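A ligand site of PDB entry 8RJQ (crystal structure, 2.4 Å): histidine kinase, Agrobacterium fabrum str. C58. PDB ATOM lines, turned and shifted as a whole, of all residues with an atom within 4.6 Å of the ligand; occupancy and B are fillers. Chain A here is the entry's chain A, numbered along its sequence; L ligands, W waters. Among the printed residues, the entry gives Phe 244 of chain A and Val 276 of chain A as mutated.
O3 of the ligand lies within salt-bridge range of NE of Arg 211 (2.7 Å). SG of Cys 13 is covalently linked to C21 of the ligand (1.9 Å). The side-chain carboxylate (OD2) of Asp 196 sits at hydrogen-bond distance from a nitrogen (N4) of the ligand (3.4 Å). An oxygen (O6) of the ligand is in hydrogen-bond range of the side-chain hydroxyl (OH) of Tyr 251 (3.0 Å). An oxygen (O2) of the ligand lies within hydrogen-bond range of a ring nitrogen (NE2) of His 248, 3.3 Å away. A ring nitrogen (NE2) of His 278 is in hydrogen-bond range of an oxygen (O2) of the ligand. O of Asp 196 lies within hydrogen-bond range of N3 of the ligand, 2.9 Å away. NH2 of Arg 242 is in salt-bridge range of O1 of the ligand (3.3 Å).
The guanidinium group of Arg 456 is in hydrogen-bond range of the side-chain hydroxyl of Ser 195, at 3.2 Å. The guanidinium group (NH2) of Arg 242 is in hydrogen-bond range of the backbone carbonyl oxygen (O) of Ile 18, 3.4 Å away. N of Ile 247 lies within hydrogen-bond range of OG of Ser 245 (3.1 Å). The side-chain carboxylate of Asp 196 is in salt-bridge range of the guanidinium group of Arg 456 (2.7 Å). OD2 of Asp 196 sits at hydrogen-bond distance from OG of Ser 462 (2.4 Å). The side-chain hydroxyl (OG) of Ser 245 lies within hydrogen-bond range of the side-chain carboxylate (OE1) of Glu 16 (2.7 Å). OH of Tyr 251 is in hydrogen-bond range of OG of Ser 462 (2.6 Å). The guanidinium group (NH1) of Arg 456 lies within hydrogen-bond range of the side-chain hydroxyl (OG) of Ser 462 (3.4 Å).
CG2 of Ile 18 touches C31 of the ligand, 3.9 Å away. CE2 of Tyr 165 touches C32 of the ligand, at 3.2 Å. CE2 of Phe 187 touches C24 of the ligand, 3.8 Å away. Phe 192 touches the ligand. Ser 195 touches the ligand. Ile 197 touches the ligand. Pro 198 touches the ligand (CD to C27, 3.2 Å). OH of Tyr 205 touches C19 of the ligand, at 3.0 Å. Ser 245 touches the ligand (CB to C31, 3.9 Å). CG2 of Ile 247 touches C9 of the ligand, at 3.8 Å. Leu 252 touches the ligand (CD2 to O2, 3.9 Å). Met 255 touches the ligand (SD to C20, 3.7 Å). CG1 of Val 276 touches O4 of the ligand, 3.2 Å away. Arg 456 touches the ligand. Leu 457 touches the ligand (CD2 to C30, 3.96 Å). Pro 459 touches the ligand (CG to C24, 3.6 Å). Ser 462 touches the ligand (CB to O6, 3.9 Å). Hydrophobic or aromatic side chains that line the ligand: Ile 18, Tyr 165, Phe 187, Phe 192, Ile 197, Pro 198, Tyr 205, Ile 247, His 248, Tyr 251, Leu 252, Met 255, Val 276, Leu 457 and Pro 459. Within 4 Å of the ligand: Cys 13, Ile 18, Tyr 165, Phe 187, Phe 192, Ser 195, Asp 196, Ile 197, Pro 198, Tyr 205, Arg 211, Arg 242, Ser 245, Ile 247, His 248, Tyr 251, Leu 252, Met 255, Val 276, His 278, Arg 456, Leu 457, Pro 459 and Ser 462. The nearest printed residue that does not touch the ligand is Ala 201 (4.1 Å).
Water W4 lies within hydrogen-bond range of the side-chain hydroxyl (OG) of Ser 260 (2.5 Å), an oxygen (O2) of the ligand (2.8 Å) and a ring nitrogen (NE2) of His 248 (3.3 Å). Water W3 bridges a ring nitrogen (ND1) of His 248 and a nitrogen (N1) of the ligand. Water W1 lies within hydrogen-bond range of O of Ser 195 and N of Asp 14.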
ATOM      1  N   CYS A  13      19.923 -35.471  -4.171  1.00  0.00           N
ATOM      2  CA  CYS A  13      20.492 -34.089  -4.192  1.00  0.00           C
ATOM      3  C   CYS A  13      19.695 -33.175  -5.131  1.00  0.00           C
ATOM      4  O   CYS A  13      19.857 -31.935  -5.039  1.00  0.00           O
ATOM      5  CB  CYS A  13      21.970 -34.093  -4.558  1.00  0.00           C
ATOM      6  SG  CYS A  13      22.328 -34.713  -6.230  1.00  0.00           S
ATOM      7  N   ASP A  14      18.877 -33.772  -6.015  1.00  0.00           N
ATOM      8  CA  ASP A  14      17.891 -33.095  -6.908  1.00  0.00           C
ATOM      9  C   ASP A  14      16.764 -32.454  -6.084  1.00  0.00           C
ATOM     10  O   ASP A  14      16.131 -31.507  -6.595  1.00  0.00           O
ATOM     11  CB  ASP A  14      17.306 -34.068  -7.925  1.00  0.00           C
ATOM     12  CG  ASP A  14      16.892 -35.403  -7.345  1.00  0.00           C
ATOM     13  OD1 ASP A  14      15.839 -35.464  -6.685  1.00  0.00           O
ATOM     14  OD2 ASP A  14      17.646 -36.392  -7.528  1.00  0.00           O
ATOM     15  N   GLU A  16      17.314 -31.728  -2.588  1.00  0.00           N
ATOM     16  CA  GLU A  16      18.007 -31.212  -1.376  1.00  0.00           C
ATOM     17  C   GLU A  16      17.427 -29.851  -0.986  1.00  0.00           C
ATOM     18  O   GLU A  16      17.360 -28.943  -1.815  1.00  0.00           O
ATOM     19  CB  GLU A  16      19.515 -31.102  -1.613  1.00  0.00           C
ATOM     20  CG  GLU A  16      20.302 -30.741  -0.367  1.00  0.00           C
ATOM     21  CD  GLU A  16      21.780 -30.474  -0.590  1.00  0.00           C
ATOM     22  OE1 GLU A  16      22.253 -30.630  -1.735  1.00  0.00           O
ATOM     23  OE2 GLU A  16      22.464 -30.092   0.383  1.00  0.00           O
ATOM     24  N   ILE A  18      18.212 -26.817   0.107  1.00  0.00           N
ATOM     25  CA  ILE A  18      19.461 -26.017   0.258  1.00  0.00           C
ATOM     26  C   ILE A  18      19.169 -24.655   0.905  1.00  0.00           C
ATOM     27  O   ILE A  18      20.130 -23.977   1.303  1.00  0.00           O
ATOM     28  CB  ILE A  18      20.171 -25.858  -1.102  1.00  0.00           C
ATOM     29  CG1 ILE A  18      19.286 -25.182  -2.155  1.00  0.00           C
ATOM     30  CG2 ILE A  18      20.695 -27.204  -1.596  1.00  0.00           C
ATOM     31  CD1 ILE A  18      20.049 -24.603  -3.319  1.00  0.00           C
ATOM     32  N   TYR A 165      27.990 -18.584 -17.981  1.00  0.00           N
ATOM     33  CA  TYR A 165      27.116 -19.704 -18.418  1.00  0.00           C
ATOM     34  C   TYR A 165      25.818 -19.116 -18.987  1.00  0.00           C
ATOM     35  O   TYR A 165      25.205 -18.275 -18.299  1.00  0.00           O
ATOM     36  CB  TYR A 165      26.751 -20.663 -17.284  1.00  0.00           C
ATOM     37  CG  TYR A 165      27.899 -21.052 -16.393  1.00  0.00           C
ATOM     38  CD1 TYR A 165      29.058 -21.587 -16.927  1.00  0.00           C
ATOM     39  CD2 TYR A 165      27.818 -20.881 -15.029  1.00  0.00           C
ATOM     40  CE1 TYR A 165      30.118 -21.954 -16.109  1.00  0.00           C
ATOM     41  CE2 TYR A 165      28.871 -21.243 -14.196  1.00  0.00           C
ATOM     42  CZ  TYR A 165      30.025 -21.783 -14.737  1.00  0.00           C
ATOM     43  OH  TYR A 165      31.052 -22.128 -13.908  1.00  0.00           O
ATOM     44  N   PHE A 187      37.297 -24.162 -19.991  1.00  0.00           N
ATOM     45  CA  PHE A 187      35.939 -24.765 -20.084  1.00  0.00           C
ATOM     46  C   PHE A 187      35.134 -24.108 -21.220  1.00  0.00           C
ATOM     47  O   PHE A 187      33.933 -24.407 -21.350  1.00  0.00           O
ATOM     48  CB  PHE A 187      35.192 -24.621 -18.749  1.00  0.00           C
ATOM     49  CG  PHE A 187      35.873 -25.270 -17.573  1.00  0.00           C
ATOM     50  CD1 PHE A 187      36.277 -26.605 -17.635  1.00  0.00           C
ATOM     51  CD2 PHE A 187      36.070 -24.571 -16.397  1.00  0.00           C
ATOM     52  CE1 PHE A 187      36.887 -27.197 -16.550  1.00  0.00           C
ATOM     53  CE2 PHE A 187      36.683 -25.175 -15.306  1.00  0.00           C
ATOM     54  CZ  PHE A 187      37.094 -26.486 -15.386  1.00  0.00           C
ATOM     55  N   PHE A 192      27.260 -28.266 -19.549  1.00  0.00           N
ATOM     56  CA  PHE A 192      26.910 -29.059 -18.345  1.00  0.00           C
ATOM     57  C   PHE A 192      25.421 -29.384 -18.385  1.00  0.00           C
ATOM     58  O   PHE A 192      24.629 -28.591 -18.891  1.00  0.00           O
ATOM     59  CB  PHE A 192      27.387 -28.374 -17.056  1.00  0.00           C
ATOM     60  CG  PHE A 192      26.829 -27.007 -16.737  1.00  0.00           C
ATOM     61  CD1 PHE A 192      25.509 -26.846 -16.312  1.00  0.00           C
ATOM     62  CD2 PHE A 192      27.638 -25.884 -16.762  1.00  0.00           C
ATOM     63  CE1 PHE A 192      25.019 -25.585 -15.980  1.00  0.00           C
ATOM     64  CE2 PHE A 192      27.143 -24.627 -16.437  1.00  0.00           C
ATOM     65  CZ  PHE A 192      25.832 -24.482 -16.036  1.00  0.00           C
ATOM     66  N   SER A 195      20.813 -31.033 -14.582  1.00  0.00           N
ATOM     67  CA  SER A 195      20.896 -31.667 -13.239  1.00  0.00           C
ATOM     68  C   SER A 195      22.061 -31.074 -12.414  1.00  0.00           C
ATOM     69  O   SER A 195      21.991 -31.165 -11.176  1.00  0.00           O
ATOM     70  CB  SER A 195      21.026 -33.165 -13.358  1.00  0.00           C
ATOM     71  OG  SER A 195      22.182 -33.509 -14.101  1.00  0.00           O
ATOM     72  N   ASP A 196      23.070 -30.489 -13.070  1.00  0.00           N
ATOM     73  CA  ASP A 196      24.240 -29.885 -12.387  1.00  0.00           C
ATOM     74  C   ASP A 196      23.832 -28.620 -11.621  1.00  0.00           C
ATOM     75  O   ASP A 196      24.635 -28.161 -10.797  1.00  0.00           O
ATOM     76  CB  ASP A 196      25.388 -29.587 -13.361  1.00  0.00           C
ATOM     77  CG  ASP A 196      26.227 -30.800 -13.689  1.00  0.00           C
ATOM     78  OD1 ASP A 196      25.725 -31.928 -13.522  1.00  0.00           O
ATOM     79  OD2 ASP A 196      27.386 -30.620 -14.115  1.00  0.00           O
ATOM     80  N   ILE A 197      22.655 -28.052 -11.889  1.00  0.00           N
ATOM     81  CA  ILE A 197      22.067 -26.922 -11.101  1.00  0.00           C
ATOM     82  C   ILE A 197      20.592 -27.229 -10.882  1.00  0.00           C
ATOM     83  O   ILE A 197      19.756 -26.897 -11.738  1.00  0.00           O
ATOM     84  CB  ILE A 197      22.310 -25.550 -11.771  1.00  0.00           C
ATOM     85  CG1 ILE A 197      23.787 -25.314 -12.084  1.00  0.00           C
ATOM     86  CG2 ILE A 197      21.731 -24.436 -10.914  1.00  0.00           C
ATOM     87  CD1 ILE A 197      24.066 -24.010 -12.821  1.00  0.00           C
ATOM     88  N   PRO A 198      20.218 -27.873  -9.758  1.00  0.00           N
ATOM     89  CA  PRO A 198      18.830 -28.204  -9.452  1.00  0.00           C
ATOM     90  C   PRO A 198      17.835 -27.035  -9.526  1.00  0.00           C
ATOM     91  O   PRO A 198      18.262 -25.888  -9.467  1.00  0.00           O
ATOM     92  CB  PRO A 198      18.894 -28.713  -8.007  1.00  0.00           C
ATOM     93  CG  PRO A 198      20.300 -29.280  -7.881  1.00  0.00           C
ATOM     94  CD  PRO A 198      21.141 -28.347  -8.722  1.00  0.00           C
ATOM     95  N   ALA A 201      17.909 -24.578  -6.642  1.00  0.00           N
ATOM     96  CA  ALA A 201      19.113 -23.726  -6.755  1.00  0.00           C
ATOM     97  C   ALA A 201      18.844 -22.571  -7.719  1.00  0.00           C
ATOM     98  O   ALA A 201      19.189 -21.424  -7.380  1.00  0.00           O
ATOM     99  CB  ALA A 201      20.304 -24.549  -7.191  1.00  0.00           C
ATOM    100  N   TYR A 205      18.857 -18.450  -7.108  1.00  0.00           N
ATOM    101  CA  TYR A 205      19.700 -17.621  -8.013  1.00  0.00           C
ATOM    102  C   TYR A 205      18.819 -16.522  -8.641  1.00  0.00           C
ATOM    103  O   TYR A 205      19.350 -15.453  -8.980  1.00  0.00           O
ATOM    104  CB  TYR A 205      20.383 -18.456  -9.108  1.00  0.00           C
ATOM    105  CG  TYR A 205      21.659 -19.144  -8.709  1.00  0.00           C
ATOM    106  CD1 TYR A 205      22.680 -18.472  -8.056  1.00  0.00           C
ATOM    107  CD2 TYR A 205      21.887 -20.477  -9.037  1.00  0.00           C
ATOM    108  CE1 TYR A 205      23.857 -19.098  -7.702  1.00  0.00           C
ATOM    109  CE2 TYR A 205      23.056 -21.124  -8.693  1.00  0.00           C
ATOM    110  CZ  TYR A 205      24.055 -20.434  -8.023  1.00  0.00           C
ATOM    111  OH  TYR A 205      25.224 -21.053  -7.668  1.00  0.00           O
ATOM    112  N   ARG A 211      25.868 -14.405  -4.878  1.00  0.00           N
ATOM    113  CA  ARG A 211      26.069 -15.664  -4.090  1.00  0.00           C
ATOM    114  C   ARG A 211      27.567 -15.831  -3.836  1.00  0.00           C
ATOM    115  O   ARG A 211      28.317 -15.877  -4.830  1.00  0.00           O
ATOM    116  CB  ARG A 211      25.449 -16.848  -4.834  1.00  0.00           C
ATOM    117  CG  ARG A 211      25.819 -18.224  -4.294  1.00  0.00           C
ATOM    118  CD  ARG A 211      25.551 -18.359  -2.807  1.00  0.00           C
ATOM    119  NE  ARG A 211      25.680 -19.732  -2.331  1.00  0.00           N
ATOM    120  CZ  ARG A 211      25.595 -20.109  -1.058  1.00  0.00           C
ATOM    121  NH1 ARG A 211      25.387 -19.203  -0.109  1.00  0.00           N
ATOM    122  NH2 ARG A 211      25.720 -21.374  -0.733  1.00  0.00           N
ATOM    123  N   ILE A 213      30.838 -17.925  -1.820  1.00  0.00           N
ATOM    124  CA  ILE A 213      31.446 -19.043  -1.039  1.00  0.00           C
ATOM    125  C   ILE A 213      32.875 -18.624  -0.692  1.00  0.00           C
ATOM    126  O   ILE A 213      33.716 -18.557  -1.610  1.00  0.00           O
ATOM    127  CB  ILE A 213      31.378 -20.370  -1.822  1.00  0.00           C
ATOM    128  CG1 ILE A 213      29.932 -20.769  -2.129  1.00  0.00           C
ATOM    129  CG2 ILE A 213      32.123 -21.469  -1.077  1.00  0.00           C
ATOM    130  CD1 ILE A 213      29.795 -22.012  -2.978  1.00  0.00           C
ATOM    131  N   ARG A 242      24.391 -18.008   4.257  1.00  0.00           N
ATOM    132  CA  ARG A 242      23.818 -19.370   4.031  1.00  0.00           C
ATOM    133  C   ARG A 242      24.928 -20.318   3.560  1.00  0.00           C
ATOM    134  O   ARG A 242      25.663 -19.952   2.626  1.00  0.00           O
ATOM    135  CB  ARG A 242      22.676 -19.307   3.013  1.00  0.00           C
ATOM    136  CG  ARG A 242      22.089 -20.660   2.631  1.00  0.00           C
ATOM    137  CD  ARG A 242      20.939 -20.523   1.644  1.00  0.00           C
ATOM    138  NE  ARG A 242      21.372 -19.913   0.392  1.00  0.00           N
ATOM    139  CZ  ARG A 242      21.901 -20.568  -0.647  1.00  0.00           C
ATOM    140  NH1 ARG A 242      22.267 -19.909  -1.734  1.00  0.00           N
ATOM    141  NH2 ARG A 242      22.061 -21.885  -0.607  1.00  0.00           N
ATOM    142  N   PHE A 244      26.583 -23.849   1.836  1.00  0.00           N
ATOM    143  CA  PHE A 244      26.444 -24.427   0.473  1.00  0.00           C
ATOM    144  C   PHE A 244      26.289 -25.943   0.595  1.00  0.00           C
ATOM    145  O   PHE A 244      26.848 -26.538   1.531  1.00  0.00           O
ATOM    146  CB  PHE A 244      27.651 -24.040  -0.391  1.00  0.00           C
ATOM    147  CG  PHE A 244      28.993 -24.161   0.287  1.00  0.00           C
ATOM    148  CD1 PHE A 244      29.438 -23.165   1.147  1.00  0.00           C
ATOM    149  CD2 PHE A 244      29.808 -25.255   0.068  1.00  0.00           C
ATOM    150  CE1 PHE A 244      30.664 -23.269   1.787  1.00  0.00           C
ATOM    151  CE2 PHE A 244      31.040 -25.354   0.702  1.00  0.00           C
ATOM    152  CZ  PHE A 244      31.468 -24.361   1.562  1.00  0.00           C
ATOM    153  N   SER A 245      25.550 -26.550  -0.349  1.00  0.00           N
ATOM    154  CA  SER A 245      25.359 -28.028  -0.435  1.00  0.00           C
ATOM    155  C   SER A 245      26.714 -28.726  -0.374  1.00  0.00           C
ATOM    156  O   SER A 245      27.654 -28.300  -1.042  1.00  0.00           O
ATOM    157  CB  SER A 245      24.617 -28.413  -1.686  1.00  0.00           C
ATOM    158  OG  SER A 245      24.761 -29.801  -1.955  1.00  0.00           O
ATOM    159  N   ILE A 247      27.368 -31.447  -1.783  1.00  0.00           N
ATOM    160  CA  ILE A 247      27.508 -32.037  -3.154  1.00  0.00           C
ATOM    161  C   ILE A 247      28.302 -31.046  -4.023  1.00  0.00           C
ATOM    162  O   ILE A 247      29.259 -31.482  -4.688  1.00  0.00           O
ATOM    163  CB  ILE A 247      26.140 -32.379  -3.770  1.00  0.00           C
ATOM    164  CG1 ILE A 247      25.402 -33.446  -2.962  1.00  0.00           C
ATOM    165  CG2 ILE A 247      26.286 -32.788  -5.232  1.00  0.00           C
ATOM    166  CD1 ILE A 247      26.103 -34.793  -2.911  1.00  0.00           C
ATOM    167  N   HIS A 248      27.914 -29.762  -3.997  1.00  0.00           N
ATOM    168  CA  HIS A 248      28.600 -28.671  -4.743  1.00  0.00           C
ATOM    169  C   HIS A 248      29.977 -28.405  -4.144  1.00  0.00           C
ATOM    170  O   HIS A 248      30.899 -28.098  -4.919  1.00  0.00           O
ATOM    171  CB  HIS A 248      27.754 -27.395  -4.764  1.00  0.00           C
ATOM    172  CG  HIS A 248      28.398 -26.300  -5.537  1.00  0.00           C
ATOM    173  ND1 HIS A 248      28.796 -26.465  -6.852  1.00  0.00           N
ATOM    174  CD2 HIS A 248      28.743 -25.035  -5.197  1.00  0.00           C
ATOM    175  CE1 HIS A 248      29.354 -25.353  -7.286  1.00  0.00           C
ATOM    176  NE2 HIS A 248      29.324 -24.455  -6.292  1.00  0.00           N
ATOM    177  N   TYR A 251      32.393 -30.843  -5.447  1.00  0.00           N
ATOM    178  CA  TYR A 251      32.598 -30.477  -6.874  1.00  0.00           C
ATOM    179  C   TYR A 251      33.747 -29.465  -6.972  1.00  0.00           C
ATOM    180  O   TYR A 251      34.689 -29.707  -7.761  1.00  0.00           O
ATOM    181  CB  TYR A 251      31.324 -29.923  -7.520  1.00  0.00           C
ATOM    182  CG  TYR A 251      31.240 -30.177  -9.005  1.00  0.00           C
ATOM    183  CD1 TYR A 251      32.134 -29.577  -9.884  1.00  0.00           C
ATOM    184  CD2 TYR A 251      30.284 -31.033  -9.534  1.00  0.00           C
ATOM    185  CE1 TYR A 251      32.076 -29.821 -11.248  1.00  0.00           C
ATOM    186  CE2 TYR A 251      30.210 -31.280 -10.898  1.00  0.00           C
ATOM    187  CZ  TYR A 251      31.110 -30.677 -11.755  1.00  0.00           C
ATOM    188  OH  TYR A 251      31.053 -30.925 -13.091  1.00  0.00           O
ATOM    189  N   LEU A 252      33.668 -28.381  -6.195  1.00  0.00           N
ATOM    190  CA  LEU A 252      34.654 -27.258  -6.232  1.00  0.00           C
ATOM    191  C   LEU A 252      36.027 -27.749  -5.780  1.00  0.00           C
ATOM    192  O   LEU A 252      37.030 -27.312  -6.377  1.00  0.00           O
ATOM    193  CB  LEU A 252      34.164 -26.116  -5.330  1.00  0.00           C
ATOM    194  CG  LEU A 252      32.917 -25.372  -5.795  1.00  0.00           C
ATOM    195  CD1 LEU A 252      32.531 -24.280  -4.802  1.00  0.00           C
ATOM    196  CD2 LEU A 252      33.095 -24.777  -7.184  1.00  0.00           C
ATOM    197  N   MET A 255      37.822 -29.688  -8.401  1.00  0.00           N
ATOM    198  CA  MET A 255      38.271 -28.767  -9.477  1.00  0.00           C
ATOM    199  C   MET A 255      39.489 -27.961  -9.004  1.00  0.00           C
ATOM    200  O   MET A 255      40.145 -27.350  -9.876  1.00  0.00           O
ATOM    201  CB  MET A 255      37.165 -27.783  -9.864  1.00  0.00           C
ATOM    202  CG  MET A 255      36.071 -28.383 -10.720  1.00  0.00           C
ATOM    203  SD  MET A 255      35.049 -27.103 -11.499  1.00  0.00           S
ATOM    204  CE  MET A 255      34.365 -26.294 -10.058  1.00  0.00           C
ATOM    205  N   SER A 260      34.293 -19.003  -4.507  1.00  0.00           N
ATOM    206  CA  SER A 260      33.476 -18.616  -5.684  1.00  0.00           C
ATOM    207  C   SER A 260      32.648 -17.372  -5.382  1.00  0.00           C
ATOM    208  O   SER A 260      32.437 -17.049  -4.186  1.00  0.00           O
ATOM    209  CB  SER A 260      32.595 -19.758  -6.131  1.00  0.00           C
ATOM    210  OG  SER A 260      31.456 -19.863  -5.296  1.00  0.00           O
ATOM    211  N   LEU A 274      24.520 -17.104 -15.520  1.00  0.00           N
ATOM    212  CA  LEU A 274      25.366 -16.650 -14.378  1.00  0.00           C
ATOM    213  C   LEU A 274      26.692 -16.118 -14.898  1.00  0.00           C
ATOM    214  O   LEU A 274      27.256 -16.739 -15.820  1.00  0.00           O
ATOM    215  CB  LEU A 274      25.617 -17.835 -13.439  1.00  0.00           C
ATOM    216  CG  LEU A 274      24.384 -18.598 -12.971  1.00  0.00           C
ATOM    217  CD1 LEU A 274      24.790 -19.853 -12.217  1.00  0.00           C
ATOM    218  CD2 LEU A 274      23.497 -17.708 -12.114  1.00  0.00           C
ATOM    219  N   VAL A 276      30.158 -16.182 -13.210  1.00  0.00           N
ATOM    220  CA  VAL A 276      30.693 -17.019 -12.098  1.00  0.00           C
ATOM    221  C   VAL A 276      32.210 -16.807 -11.987  1.00  0.00           C
ATOM    222  O   VAL A 276      32.917 -17.108 -12.957  1.00  0.00           O
ATOM    223  CB  VAL A 276      30.343 -18.499 -12.316  1.00  0.00           C
ATOM    224  CG1 VAL A 276      31.128 -19.409 -11.384  1.00  0.00           C
ATOM    225  CG2 VAL A 276      28.856 -18.717 -12.179  1.00  0.00           C
ATOM    226  N   HIS A 278      35.637 -17.985 -10.000  1.00  0.00           N
ATOM    227  CA  HIS A 278      36.320 -19.065  -9.237  1.00  0.00           C
ATOM    228  C   HIS A 278      37.685 -18.560  -8.750  1.00  0.00           C
ATOM    229  O   HIS A 278      38.386 -17.901  -9.531  1.00  0.00           O
ATOM    230  CB  HIS A 278      36.498 -20.326 -10.089  1.00  0.00           C
ATOM    231  CG  HIS A 278      35.237 -21.096 -10.328  1.00  0.00           C
ATOM    232  ND1 HIS A 278      35.150 -22.060 -11.314  1.00  0.00           N
ATOM    233  CD2 HIS A 278      34.032 -21.044  -9.735  1.00  0.00           C
ATOM    234  CE1 HIS A 278      33.941 -22.581 -11.301  1.00  0.00           C
ATOM    235  NE2 HIS A 278      33.232 -21.972 -10.341  1.00  0.00           N
ATOM    236  N   ARG A 456      31.357 -38.451 -10.755  1.00  0.00           N
ATOM    237  CA  ARG A 456      30.162 -37.704 -11.256  1.00  0.00           C
ATOM    238  C   ARG A 456      30.360 -36.197 -11.031  1.00  0.00           C
ATOM    239  O   ARG A 456      29.851 -35.406 -11.857  1.00  0.00           O
ATOM    240  CB  ARG A 456      28.893 -38.190 -10.560  1.00  0.00           C
ATOM    241  CG  ARG A 456      27.642 -37.364 -10.828  1.00  0.00           C
ATOM    242  CD  ARG A 456      27.262 -37.317 -12.296  1.00  0.00           C
ATOM    243  NE  ARG A 456      26.106 -36.468 -12.535  1.00  0.00           N
ATOM    244  CZ  ARG A 456      26.143 -35.157 -12.809  1.00  0.00           C
ATOM    245  NH1 ARG A 456      27.300 -34.521 -12.877  1.00  0.00           N
ATOM    246  NH2 ARG A 456      25.019 -34.500 -13.003  1.00  0.00           N
ATOM    247  N   LEU A 457      31.051 -35.824  -9.951  1.00  0.00           N
ATOM    248  CA  LEU A 457      31.260 -34.406  -9.552  1.00  0.00           C
ATOM    249  C   LEU A 457      32.576 -33.887 -10.139  1.00  0.00           C
ATOM    250  O   LEU A 457      33.408 -33.361  -9.371  1.00  0.00           O
ATOM    251  CB  LEU A 457      31.239 -34.331  -8.016  1.00  0.00           C
ATOM    252  CG  LEU A 457      30.009 -34.960  -7.346  1.00  0.00           C
ATOM    253  CD1 LEU A 457      30.043 -34.748  -5.843  1.00  0.00           C
ATOM    254  CD2 LEU A 457      28.720 -34.390  -7.925  1.00  0.00           C
ATOM    255  N   PRO A 459      33.979 -31.769 -14.015  1.00  0.00           N
ATOM    256  CA  PRO A 459      33.642 -31.219 -15.326  1.00  0.00           C
ATOM    257  C   PRO A 459      33.706 -32.229 -16.493  1.00  0.00           C
ATOM    258  O   PRO A 459      32.885 -32.123 -17.393  1.00  0.00           O
ATOM    259  CB  PRO A 459      34.713 -30.142 -15.528  1.00  0.00           C
ATOM    260  CG  PRO A 459      35.019 -29.669 -14.127  1.00  0.00           C
ATOM    261  CD  PRO A 459      34.930 -30.921 -13.280  1.00  0.00           C
ATOM    262  N   SER A 462      30.472 -34.456 -16.179  1.00  0.00           N
ATOM    263  CA  SER A 462      29.337 -33.532 -16.473  1.00  0.00           C
ATOM    264  C   SER A 462      29.173 -33.411 -17.994  1.00  0.00           C
ATOM    265  O   SER A 462      28.048 -33.616 -18.492  1.00  0.00           O
ATOM    266  CB  SER A 462      29.531 -32.184 -15.826  1.00  0.00           C
ATOM    267  OG  SER A 462      29.185 -32.223 -14.446  1.00  0.00           O
HETATM  268  C1  LIG L   1      26.059 -31.209  -9.387  1.00  0.00           C
HETATM  269  C2  LIG L   1      24.099 -28.014  -7.113  1.00  0.00           C
HETATM  270  O1  LIG L   1      24.002 -23.313  -2.880  1.00  0.00           O
HETATM  271  C3  LIG L   1      26.464 -25.104  -9.250  1.00  0.00           C
HETATM  272  O2  LIG L   1      30.400 -22.445  -8.684  1.00  0.00           O
HETATM  273  C4  LIG L   1      29.124 -26.867 -12.761  1.00  0.00           C
HETATM  274  C5  LIG L   1      25.124 -32.142  -8.999  1.00  0.00           C
HETATM  275  C6  LIG L   1      23.657 -27.176  -6.088  1.00  0.00           C
HETATM  276  O3  LIG L   1      25.655 -22.081  -3.690  1.00  0.00           O
HETATM  277  C7  LIG L   1      26.923 -24.031 -10.007  1.00  0.00           C
HETATM  278  O4  LIG L   1      29.531 -22.092 -10.656  1.00  0.00           O
HETATM  279  C8  LIG L   1      30.308 -26.126 -12.759  1.00  0.00           C
HETATM  280  C9  LIG L   1      24.156 -31.647  -8.133  1.00  0.00           C
HETATM  281  C10 LIG L   1      24.236 -25.930  -6.305  1.00  0.00           C
HETATM  282  C11 LIG L   1      27.445 -24.526 -11.182  1.00  0.00           C
HETATM  283  C12 LIG L   1      31.185 -26.724 -13.678  1.00  0.00           C
HETATM  284  C13 LIG L   1      24.498 -30.306  -8.019  1.00  0.00           C
HETATM  285  C14 LIG L   1      24.994 -26.044  -7.466  1.00  0.00           C
HETATM  286  C15 LIG L   1      27.324 -25.914 -11.180  1.00  0.00           C
HETATM  287  C16 LIG L   1      30.549 -27.826 -14.219  1.00  0.00           C
HETATM  288  C17 LIG L   1      23.033 -32.344  -7.618  1.00  0.00           C
HETATM  289  C18 LIG L   1      24.055 -24.682  -5.483  1.00  0.00           C
HETATM  290  C19 LIG L   1      26.877 -22.571  -9.632  1.00  0.00           C
HETATM  291  C20 LIG L   1      32.479 -26.269 -14.016  1.00  0.00           C
HETATM  292  C21 LIG L   1      22.870 -33.665  -7.677  1.00  0.00           C
HETATM  293  C22 LIG L   1      25.275 -24.218  -4.677  1.00  0.00           C
HETATM  294  C23 LIG L   1      28.043 -22.067  -8.797  1.00  0.00           C
HETATM  295  C24 LIG L   1      33.220 -26.655 -15.054  1.00  0.00           C
HETATM  296  C25 LIG L   1      24.948 -23.125  -3.671  1.00  0.00           C
HETATM  297  C26 LIG L   1      29.421 -22.222  -9.437  1.00  0.00           C
HETATM  298  C27 LIG L   1      23.787 -29.355  -7.300  1.00  0.00           C
HETATM  299  C28 LIG L   1      25.781 -25.048  -8.042  1.00  0.00           C
HETATM  300  C29 LIG L   1      27.869 -26.737 -12.163  1.00  0.00           C
HETATM  301  C30 LIG L   1      25.175 -33.566  -9.477  1.00  0.00           C
HETATM  302  C31 LIG L   1      22.744 -27.530  -4.948  1.00  0.00           C
HETATM  303  C32 LIG L   1      28.045 -23.718 -12.284  1.00  0.00           C
HETATM  304  C33 LIG L   1      30.679 -24.903 -11.976  1.00  0.00           C
HETATM  305  N1  LIG L   1      25.656 -30.033  -8.761  1.00  0.00           N
HETATM  306  O5  LIG L   1      27.010 -31.349 -10.106  1.00  0.00           O
HETATM  307  N2  LIG L   1      24.890 -27.307  -7.969  1.00  0.00           N
HETATM  308  N3  LIG L   1      26.656 -26.231 -10.014  1.00  0.00           N
HETATM  309  N4  LIG L   1      29.307 -27.911 -13.656  1.00  0.00           N
HETATM  310  O6  LIG L   1      30.986 -28.609 -15.058  1.00  0.00           O
HETATM  311  O   HOH W   1      20.222 -33.304  -9.190  1.00  0.00           O
HETATM  312  O   HOH W   2      30.810 -29.052 -17.835  1.00  0.00           O
HETATM  313  O   HOH W   3      28.261 -28.590  -8.312  1.00  0.00           O
HETATM  314  O   HOH W   4      29.568 -21.180  -6.388  1.00  0.00           O
